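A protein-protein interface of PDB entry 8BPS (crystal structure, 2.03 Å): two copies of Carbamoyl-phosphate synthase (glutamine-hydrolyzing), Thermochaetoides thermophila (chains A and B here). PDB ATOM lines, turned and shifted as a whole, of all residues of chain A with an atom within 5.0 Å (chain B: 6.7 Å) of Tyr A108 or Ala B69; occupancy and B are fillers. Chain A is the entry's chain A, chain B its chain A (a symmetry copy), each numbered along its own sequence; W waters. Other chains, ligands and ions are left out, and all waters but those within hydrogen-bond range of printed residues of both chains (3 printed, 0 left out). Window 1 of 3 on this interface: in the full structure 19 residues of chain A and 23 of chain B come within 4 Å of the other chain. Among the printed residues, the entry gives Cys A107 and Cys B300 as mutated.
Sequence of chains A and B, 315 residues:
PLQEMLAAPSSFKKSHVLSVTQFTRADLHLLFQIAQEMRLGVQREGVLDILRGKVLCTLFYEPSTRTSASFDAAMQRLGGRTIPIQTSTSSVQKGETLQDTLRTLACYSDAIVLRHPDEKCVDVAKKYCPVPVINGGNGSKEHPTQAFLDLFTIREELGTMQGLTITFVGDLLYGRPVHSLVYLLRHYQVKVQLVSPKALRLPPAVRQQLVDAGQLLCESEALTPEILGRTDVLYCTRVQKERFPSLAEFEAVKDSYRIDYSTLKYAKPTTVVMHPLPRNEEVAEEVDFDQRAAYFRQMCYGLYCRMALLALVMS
The side-chain hydroxyl of Thr A104 is in hydrogen-bond range of the guanidinium group of Arg B66 (3.3 Å). The side-chain sulfur (SG) of Cys A107 forms a disulfide with the side-chain sulfur (SG) of Cys B300, 2.1 Å away. The side-chain carboxylate of Asp A110 lies within salt-bridge range of the guanidinium group of Arg B77. The side-chain hydroxyl of Tyr A108 sits at hydrogen-bond distance from the backbone carbonyl oxygen of Arg B66, 2.9 Å away. The guanidinium group of Arg B77 lies within hydrogen-bond range of the backbone carbonyl oxygen of Tyr A108, 3.0 Å away.
OG of Ser A109 is in hydrogen-bond range of O of Leu A105, at 3.1 Å. O of Val A55 is in hydrogen-bond range of N of Asp A110. The side-chain hydroxyl (OG) of Ser B70 sits at hydrogen-bond distance from the guanidinium group (NH1) of Arg B306 (3.0 Å).
Val A55 touches Arg B77 (CG2 to NH2, 3.5 Å). Asp B72 touches Ile A83 (OD2 to CG2, 3.7 Å). Ala B73 touches Ile A83 (CB to CD1, 3.4 Å). OG1 of Thr B65 touches CG2 of Ile A85 (3.9 Å). Ala B69 touches Ile A85 (CB to CD1, 3.9 Å). CG2 of Thr A104 touches SD of Met B299, at 3.8 Å. Thr B65 touches Leu A105 (CG2 to CD2, 3.99 Å). Cys A107 touches Met B299. CD2 of Tyr A108 touches C of Ala B69, at 3.9 Å. Tyr A108 touches Ala B73 (CB to CB, 3.7 Å).
Of the printed residues of chain B, Leu A105 touches Thr B65 (3.99 Å) and Ala B69 (3.9 Å). Thr B58 touches none of the printed residues of chain A. Ala B69 touches three residues of chain A. Of the printed residues of chain A, Leu B303 touches Cys A107 (3.5 Å). The nearest printed residue of chain B that does not touch Tyr A108 is Leu B303 (4.4 Å). The nearest residue of chain A that does not touch Ala B69 is Ile A83 (4.1 Å).
Of the 19 printed residues of chain B, 10 touch a printed residue of chain A. Of the 10 printed residues of chain A, 9 touch a printed residue of chain B. Among the printed residues, 20 pairs touch across the chains.
No position is printed for both chains.
Water W3 lies within hydrogen-bond range of the backbone carbonyl oxygen of Cys A107 (2.6 Å) and the side-chain sulfur of Cys B300 (2.9 Å). Water W1 bridges the guanidinium group (NH1) of Arg B77 (2.6 Å) and the side-chain carboxylate (OD2) of Asp A110 (2.8 Å). Water W2 lies within hydrogen-bond range of the side-chain hydroxyl (OG) of Ser B70 (2.8 Å), the backbone carbonyl oxygen (O) of Met B299 (2.8 Å), the guanidinium group (NH1) of Arg B306 (3.1 Å) and the side-chain hydroxyl (OH) of Tyr A108 (3.2 Å).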
ATOM      1  N   VAL A  55      18.419  23.034  -0.793  1.00  0.00           N
ATOM      2  CA  VAL A  55      18.516  22.627  -2.195  1.00  0.00           C
ATOM      3  C   VAL A  55      18.023  21.191  -2.317  1.00  0.00           C
ATOM      4  O   VAL A  55      18.506  20.307  -1.605  1.00  0.00           O
ATOM      5  CB  VAL A  55      19.961  22.748  -2.713  1.00  0.00           C
ATOM      6  CG1 VAL A  55      20.062  22.358  -4.186  1.00  0.00           C
ATOM      7  CG2 VAL A  55      20.505  24.162  -2.433  1.00  0.00           C
ATOM      8  N   ILE A  83      17.368  21.297  -8.278  1.00  0.00           N
ATOM      9  CA  ILE A  83      18.290  20.887  -9.337  1.00  0.00           C
ATOM     10  C   ILE A  83      17.704  19.630  -9.968  1.00  0.00           C
ATOM     11  O   ILE A  83      17.902  18.516  -9.458  1.00  0.00           O
ATOM     12  CB  ILE A  83      19.719  20.644  -8.821  1.00  0.00           C
ATOM     13  CG1 ILE A  83      20.282  21.938  -8.217  1.00  0.00           C
ATOM     14  CG2 ILE A  83      20.592  20.087  -9.983  1.00  0.00           C
ATOM     15  CD1 ILE A  83      21.404  21.700  -7.275  1.00  0.00           C
ATOM     16  N   ILE A  85      17.676  16.615 -12.328  1.00  0.00           N
ATOM     17  CA  ILE A  85      18.694  15.887 -13.080  1.00  0.00           C
ATOM     18  C   ILE A  85      18.056  15.356 -14.357  1.00  0.00           C
ATOM     19  O   ILE A  85      17.028  14.665 -14.305  1.00  0.00           O
ATOM     20  CB  ILE A  85      19.307  14.748 -12.256  1.00  0.00           C
ATOM     21  CG1 ILE A  85      20.005  15.282 -11.004  1.00  0.00           C
ATOM     22  CG2 ILE A  85      20.253  13.932 -13.141  1.00  0.00           C
ATOM     23  CD1 ILE A  85      20.927  16.438 -11.233  1.00  0.00           C
ATOM     24  N   THR A 104      27.308  11.400  -5.237  1.00  0.00           N
ATOM     25  CA  THR A 104      27.687  12.614  -5.952  1.00  0.00           C
ATOM     26  C   THR A 104      26.699  13.750  -5.668  1.00  0.00           C
ATOM     27  O   THR A 104      27.091  14.851  -5.241  1.00  0.00           O
ATOM     28  CB  THR A 104      27.733  12.312  -7.458  1.00  0.00           C
ATOM     29  OG1 THR A 104      28.811  11.407  -7.778  1.00  0.00           O
ATOM     30  CG2 THR A 104      27.918  13.552  -8.233  1.00  0.00           C
ATOM     31  N   LEU A 105      25.400  13.496  -5.904  1.00  0.00           N
ATOM     32  CA  LEU A 105      24.400  14.547  -5.762  1.00  0.00           C
ATOM     33  C   LEU A 105      24.218  14.947  -4.308  1.00  0.00           C
ATOM     34  O   LEU A 105      23.857  16.101  -4.034  1.00  0.00           O
ATOM     35  CB  LEU A 105      23.063  14.110  -6.364  1.00  0.00           C
ATOM     36  CG  LEU A 105      23.103  13.889  -7.878  1.00  0.00           C
ATOM     37  CD1 LEU A 105      21.787  13.345  -8.311  1.00  0.00           C
ATOM     38  CD2 LEU A 105      23.441  15.196  -8.620  1.00  0.00           C
ATOM     39  N   ALA A 106      24.484  14.024  -3.366  1.00  0.00           N
ATOM     40  CA  ALA A 106      24.433  14.381  -1.949  1.00  0.00           C
ATOM     41  C   ALA A 106      25.454  15.458  -1.590  1.00  0.00           C
ATOM     42  O   ALA A 106      25.275  16.152  -0.582  1.00  0.00           O
ATOM     43  CB  ALA A 106      24.681  13.148  -1.076  1.00  0.00           C
ATOM     44  N   CYS A 107      26.528  15.611  -2.368  1.00  0.00           N
ATOM     45  CA  CYS A 107      27.473  16.705  -2.123  1.00  0.00           C
ATOM     46  C   CYS A 107      26.935  18.067  -2.558  1.00  0.00           C
ATOM     47  O   CYS A 107      27.552  19.091  -2.240  1.00  0.00           O
ATOM     48  CB  CYS A 107      28.796  16.457  -2.858  1.00  0.00           C
ATOM     49  SG  CYS A 107      29.934  15.393  -1.983  1.00  0.00           S
ATOM     50  N   TYR A 108      25.825  18.106  -3.298  1.00  0.00           N
ATOM     51  CA  TYR A 108      25.278  19.349  -3.820  1.00  0.00           C
ATOM     52  C   TYR A 108      23.970  19.780  -3.183  1.00  0.00           C
ATOM     53  O   TYR A 108      23.669  20.974  -3.164  1.00  0.00           O
ATOM     54  CB  TYR A 108      25.030  19.213  -5.339  1.00  0.00           C
ATOM     55  CG  TYR A 108      26.217  18.660  -6.105  1.00  0.00           C
ATOM     56  CD1 TYR A 108      27.529  18.876  -5.669  1.00  0.00           C
ATOM     57  CD2 TYR A 108      26.031  17.933  -7.260  1.00  0.00           C
ATOM     58  CE1 TYR A 108      28.616  18.382  -6.392  1.00  0.00           C
ATOM     59  CE2 TYR A 108      27.102  17.433  -7.977  1.00  0.00           C
ATOM     60  CZ  TYR A 108      28.388  17.663  -7.542  1.00  0.00           C
ATOM     61  OH  TYR A 108      29.426  17.147  -8.262  1.00  0.00           O
ATOM     62  N   SER A 109      23.158  18.830  -2.733  1.00  0.00           N
ATOM     63  CA  SER A 109      21.790  19.077  -2.316  1.00  0.00           C
ATOM     64  C   SER A 109      21.604  18.563  -0.892  1.00  0.00           C
ATOM     65  O   SER A 109      22.443  17.839  -0.355  1.00  0.00           O
ATOM     66  CB  SER A 109      20.781  18.402  -3.276  1.00  0.00           C
ATOM     67  OG  SER A 109      21.012  17.007  -3.320  1.00  0.00           O
ATOM     68  N   ASP A 110      20.511  18.985  -0.268  1.00  0.00           N
ATOM     69  CA  ASP A 110      20.203  18.615   1.108  1.00  0.00           C
ATOM     70  C   ASP A 110      19.238  17.449   1.170  1.00  0.00           C
ATOM     71  O   ASP A 110      19.052  16.861   2.241  1.00  0.00           O
ATOM     72  CB  ASP A 110      19.648  19.832   1.870  1.00  0.00           C
ATOM     73  CG  ASP A 110      20.562  21.055   1.738  1.00  0.00           C
ATOM     74  OD1 ASP A 110      21.724  20.953   2.192  1.00  0.00           O
ATOM     75  OD2 ASP A 110      20.145  22.095   1.175  1.00  0.00           O
ATOM     76  N   THR B  58      24.016  26.534 -18.309  1.00  0.00           N
ATOM     77  CA  THR B  58      24.841  25.346 -18.451  1.00  0.00           C
ATOM     78  C   THR B  58      24.451  24.694 -19.761  1.00  0.00           C
ATOM     79  O   THR B  58      23.258  24.508 -20.039  1.00  0.00           O
ATOM     80  CB  THR B  58      24.698  24.375 -17.273  1.00  0.00           C
ATOM     81  OG1 THR B  58      23.326  24.069 -17.057  1.00  0.00           O
ATOM     82  CG2 THR B  58      25.281  25.034 -16.037  1.00  0.00           C
ATOM     83  N   PHE B  60      25.565  21.603 -22.011  1.00  0.00           N
ATOM     84  CA  PHE B  60      26.290  20.333 -22.040  1.00  0.00           C
ATOM     85  C   PHE B  60      25.806  19.547 -23.257  1.00  0.00           C
ATOM     86  O   PHE B  60      24.650  19.093 -23.292  1.00  0.00           O
ATOM     87  CB  PHE B  60      26.075  19.563 -20.737  1.00  0.00           C
ATOM     88  CG  PHE B  60      26.956  20.024 -19.615  1.00  0.00           C
ATOM     89  CD1 PHE B  60      26.856  21.319 -19.137  1.00  0.00           C
ATOM     90  CD2 PHE B  60      27.933  19.193 -19.088  1.00  0.00           C
ATOM     91  CE1 PHE B  60      27.681  21.768 -18.096  1.00  0.00           C
ATOM     92  CE2 PHE B  60      28.753  19.638 -18.066  1.00  0.00           C
ATOM     93  CZ  PHE B  60      28.623  20.931 -17.569  1.00  0.00           C
ATOM     94  N   SER B  64      27.108  15.171 -18.307  1.00  0.00           N
ATOM     95  CA  SER B  64      28.036  14.885 -17.210  1.00  0.00           C
ATOM     96  C   SER B  64      27.309  15.379 -15.962  1.00  0.00           C
ATOM     97  O   SER B  64      27.479  16.530 -15.553  1.00  0.00           O
ATOM     98  CB  SER B  64      29.405  15.538 -17.339  1.00  0.00           C
ATOM     99  OG  SER B  64      30.192  15.278 -16.148  1.00  0.00           O
ATOM    100  N   THR B  65      26.456  14.511 -15.396  1.00  0.00           N
ATOM    101  CA  THR B  65      25.679  14.913 -14.222  1.00  0.00           C
ATOM    102  C   THR B  65      26.590  15.478 -13.126  1.00  0.00           C
ATOM    103  O   THR B  65      26.275  16.502 -12.518  1.00  0.00           O
ATOM    104  CB  THR B  65      24.846  13.730 -13.713  1.00  0.00           C
ATOM    105  OG1 THR B  65      23.787  13.454 -14.649  1.00  0.00           O
ATOM    106  CG2 THR B  65      24.230  14.009 -12.342  1.00  0.00           C
ATOM    107  N   ARG B  66      27.739  14.845 -12.881  1.00  0.00           N
ATOM    108  CA  ARG B  66      28.593  15.303 -11.788  1.00  0.00           C
ATOM    109  C   ARG B  66      29.084  16.726 -12.034  1.00  0.00           C
ATOM    110  O   ARG B  66      29.184  17.529 -11.101  1.00  0.00           O
ATOM    111  CB  ARG B  66      29.771  14.347 -11.581  1.00  0.00           C
ATOM    112  CG  ARG B  66      30.953  14.558 -12.500  1.00  0.00           C
ATOM    113  CD  ARG B  66      31.994  13.458 -12.280  1.00  0.00           C
ATOM    114  NE  ARG B  66      31.537  12.508 -11.268  1.00  0.00           N
ATOM    115  CZ  ARG B  66      30.852  11.412 -11.554  1.00  0.00           C
ATOM    116  NH1 ARG B  66      30.646  11.043 -12.810  1.00  0.00           N
ATOM    117  NH2 ARG B  66      30.348  10.682 -10.557  1.00  0.00           N
ATOM    118  N   THR B  67      29.391  17.064 -13.285  1.00  0.00           N
ATOM    119  CA  THR B  67      29.864  18.411 -13.583  1.00  0.00           C
ATOM    120  C   THR B  67      28.720  19.426 -13.668  1.00  0.00           C
ATOM    121  O   THR B  67      28.762  20.478 -13.013  1.00  0.00           O
ATOM    122  CB  THR B  67      30.652  18.385 -14.892  1.00  0.00           C
ATOM    123  OG1 THR B  67      31.681  17.393 -14.802  1.00  0.00           O
ATOM    124  CG2 THR B  67      31.291  19.724 -15.181  1.00  0.00           C
ATOM    125  N   SER B  68      27.679  19.121 -14.449  1.00  0.00           N
ATOM    126  CA  SER B  68      26.614  20.101 -14.664  1.00  0.00           C
ATOM    127  C   SER B  68      25.863  20.389 -13.369  1.00  0.00           C
ATOM    128  O   SER B  68      25.579  21.552 -13.060  1.00  0.00           O
ATOM    129  CB  SER B  68      25.655  19.619 -15.759  1.00  0.00           C
ATOM    130  OG  SER B  68      25.018  18.403 -15.388  1.00  0.00           O
ATOM    131  N   ALA B  69      25.552  19.355 -12.580  1.00  0.00           N
ATOM    132  CA  ALA B  69      24.818  19.624 -11.347  1.00  0.00           C
ATOM    133  C   ALA B  69      25.696  20.347 -10.341  1.00  0.00           C
ATOM    134  O   ALA B  69      25.185  21.158  -9.562  1.00  0.00           O
ATOM    135  CB  ALA B  69      24.252  18.341 -10.752  1.00  0.00           C
ATOM    136  N   SER B  70      27.014  20.081 -10.351  1.00  0.00           N
ATOM    137  CA  SER B  70      27.921  20.818  -9.475  1.00  0.00           C
ATOM    138  C   SER B  70      27.857  22.309  -9.780  1.00  0.00           C
ATOM    139  O   SER B  70      27.720  23.130  -8.872  1.00  0.00           O
ATOM    140  CB  SER B  70      29.351  20.287  -9.626  1.00  0.00           C
ATOM    141  OG  SER B  70      30.232  21.001  -8.791  1.00  0.00           O
ATOM    142  N   PHE B  71      27.955  22.680 -11.063  1.00  0.00           N
ATOM    143  CA  PHE B  71      27.875  24.096 -11.426  1.00  0.00           C
ATOM    144  C   PHE B  71      26.501  24.684 -11.100  1.00  0.00           C
ATOM    145  O   PHE B  71      26.406  25.840 -10.664  1.00  0.00           O
ATOM    146  CB  PHE B  71      28.190  24.289 -12.915  1.00  0.00           C
ATOM    147  CG  PHE B  71      29.667  24.383 -13.224  1.00  0.00           C
ATOM    148  CD1 PHE B  71      30.397  25.513 -12.882  1.00  0.00           C
ATOM    149  CD2 PHE B  71      30.329  23.332 -13.843  1.00  0.00           C
ATOM    150  CE1 PHE B  71      31.752  25.606 -13.159  1.00  0.00           C
ATOM    151  CE2 PHE B  71      31.735  23.414 -14.117  1.00  0.00           C
ATOM    152  CZ  PHE B  71      32.421  24.553 -13.790  1.00  0.00           C
ATOM    153  N   ASP B  72      25.424  23.945 -11.380  1.00  0.00           N
ATOM    154  CA  ASP B  72      24.082  24.433 -11.060  1.00  0.00           C
ATOM    155  C   ASP B  72      23.961  24.724  -9.562  1.00  0.00           C
ATOM    156  O   ASP B  72      23.572  25.827  -9.139  1.00  0.00           O
ATOM    157  CB  ASP B  72      23.057  23.382 -11.496  1.00  0.00           C
ATOM    158  CG  ASP B  72      21.633  23.897 -11.467  1.00  0.00           C
ATOM    159  OD1 ASP B  72      21.403  24.982 -10.915  1.00  0.00           O
ATOM    160  OD2 ASP B  72      20.722  23.197 -11.971  1.00  0.00           O
ATOM    161  N   ALA B  73      24.367  23.761  -8.740  1.00  0.00           N
ATOM    162  CA  ALA B  73      24.266  23.930  -7.295  1.00  0.00           C
ATOM    163  C   ALA B  73      25.184  25.040  -6.790  1.00  0.00           C
ATOM    164  O   ALA B  73      24.810  25.795  -5.880  1.00  0.00           O
ATOM    165  CB  ALA B  73      24.580  22.606  -6.610  1.00  0.00           C
ATOM    166  N   ALA B  74      26.382  25.169  -7.361  1.00  0.00           N
ATOM    167  CA  ALA B  74      27.270  26.234  -6.916  1.00  0.00           C
ATOM    168  C   ALA B  74      26.647  27.591  -7.204  1.00  0.00           C
ATOM    169  O   ALA B  74      26.543  28.448  -6.315  1.00  0.00           O
ATOM    170  CB  ALA B  74      28.639  26.113  -7.589  1.00  0.00           C
ATOM    171  N   ARG B  77      23.693  28.147  -4.903  1.00  0.00           N
ATOM    172  CA  ARG B  77      24.100  28.427  -3.525  1.00  0.00           C
ATOM    173  C   ARG B  77      24.822  29.762  -3.394  1.00  0.00           C
ATOM    174  O   ARG B  77      24.996  30.253  -2.264  1.00  0.00           O
ATOM    175  CB  ARG B  77      24.968  27.287  -2.991  1.00  0.00           C
ATOM    176  CG  ARG B  77      24.148  26.020  -2.686  1.00  0.00           C
ATOM    177  CD  ARG B  77      24.994  24.944  -2.006  1.00  0.00           C
ATOM    178  NE  ARG B  77      24.260  23.714  -1.753  1.00  0.00           N
ATOM    179  CZ  ARG B  77      23.458  23.521  -0.716  1.00  0.00           C
ATOM    180  NH1 ARG B  77      23.267  24.468   0.193  1.00  0.00           N
ATOM    181  NH2 ARG B  77      22.829  22.352  -0.591  1.00  0.00           N
ATOM    182  N   MET B 299      33.926  15.574  -4.716  1.00  0.00           N
ATOM    183  CA  MET B 299      32.769  16.257  -5.278  1.00  0.00           C
ATOM    184  C   MET B 299      32.344  17.423  -4.394  1.00  0.00           C
ATOM    185  O   MET B 299      31.955  18.485  -4.908  1.00  0.00           O
ATOM    186  CB  MET B 299      31.586  15.278  -5.413  1.00  0.00           C
ATOM    187  CG  MET B 299      31.956  13.969  -6.080  1.00  0.00           C
ATOM    188  SD  MET B 299      31.673  14.049  -7.790  1.00  0.00           S
ATOM    189  CE  MET B 299      33.214  14.746  -8.376  1.00  0.00           C
ATOM    190  N   CYS B 300      32.321  17.209  -3.068  1.00  0.00           N
ATOM    191  CA  CYS B 300      32.014  18.296  -2.149  1.00  0.00           C
ATOM    192  C   CYS B 300      33.031  19.417  -2.293  1.00  0.00           C
ATOM    193  O   CYS B 300      32.655  20.590  -2.406  1.00  0.00           O
ATOM    194  CB  CYS B 300      31.946  17.771  -0.704  1.00  0.00           C
ATOM    195  SG  CYS B 300      30.529  16.630  -0.417  1.00  0.00           S
ATOM    196  N   GLY B 302      34.701  20.133  -4.937  1.00  0.00           N
ATOM    197  CA  GLY B 302      34.397  20.785  -6.207  1.00  0.00           C
ATOM    198  C   GLY B 302      33.281  21.814  -6.114  1.00  0.00           C
ATOM    199  O   GLY B 302      33.303  22.838  -6.806  1.00  0.00           O
ATOM    200  N   LEU B 303      32.314  21.588  -5.235  1.00  0.00           N
ATOM    201  CA  LEU B 303      31.224  22.549  -5.115  1.00  0.00           C
ATOM    202  C   LEU B 303      31.760  23.896  -4.657  1.00  0.00           C
ATOM    203  O   LEU B 303      31.454  24.932  -5.255  1.00  0.00           O
ATOM    204  CB  LEU B 303      30.161  22.028  -4.147  1.00  0.00           C
ATOM    205  CG  LEU B 303      29.050  23.008  -3.787  1.00  0.00           C
ATOM    206  CD1 LEU B 303      28.100  23.235  -4.974  1.00  0.00           C
ATOM    207  CD2 LEU B 303      28.257  22.490  -2.573  1.00  0.00           C
ATOM    208  N   ARG B 306      33.961  25.585  -7.273  1.00  0.00           N
ATOM    209  CA  ARG B 306      33.191  26.202  -8.353  1.00  0.00           C
ATOM    210  C   ARG B 306      32.372  27.393  -7.855  1.00  0.00           C
ATOM    211  O   ARG B 306      32.139  28.339  -8.619  1.00  0.00           O
ATOM    212  CB  ARG B 306      32.283  25.165  -9.022  1.00  0.00           C
ATOM    213  CG  ARG B 306      33.076  24.284  -9.929  1.00  0.00           C
ATOM    214  CD  ARG B 306      32.355  23.027 -10.424  1.00  0.00           C
ATOM    215  NE  ARG B 306      33.245  22.269 -11.288  1.00  0.00           N
ATOM    216  CZ  ARG B 306      33.321  20.948 -11.324  1.00  0.00           C
ATOM    217  NH1 ARG B 306      32.615  20.189 -10.496  1.00  0.00           N
ATOM    218  NH2 ARG B 306      34.144  20.376 -12.196  1.00  0.00           N
HETATM  219  O   HOH W   1      21.778  24.027   2.331  1.00  0.00           O
HETATM  220  O   HOH W   2      31.880  19.049  -7.685  1.00  0.00           O
HETATM  221  O   HOH W   3      29.252  19.201  -0.238  1.00  0.00           O
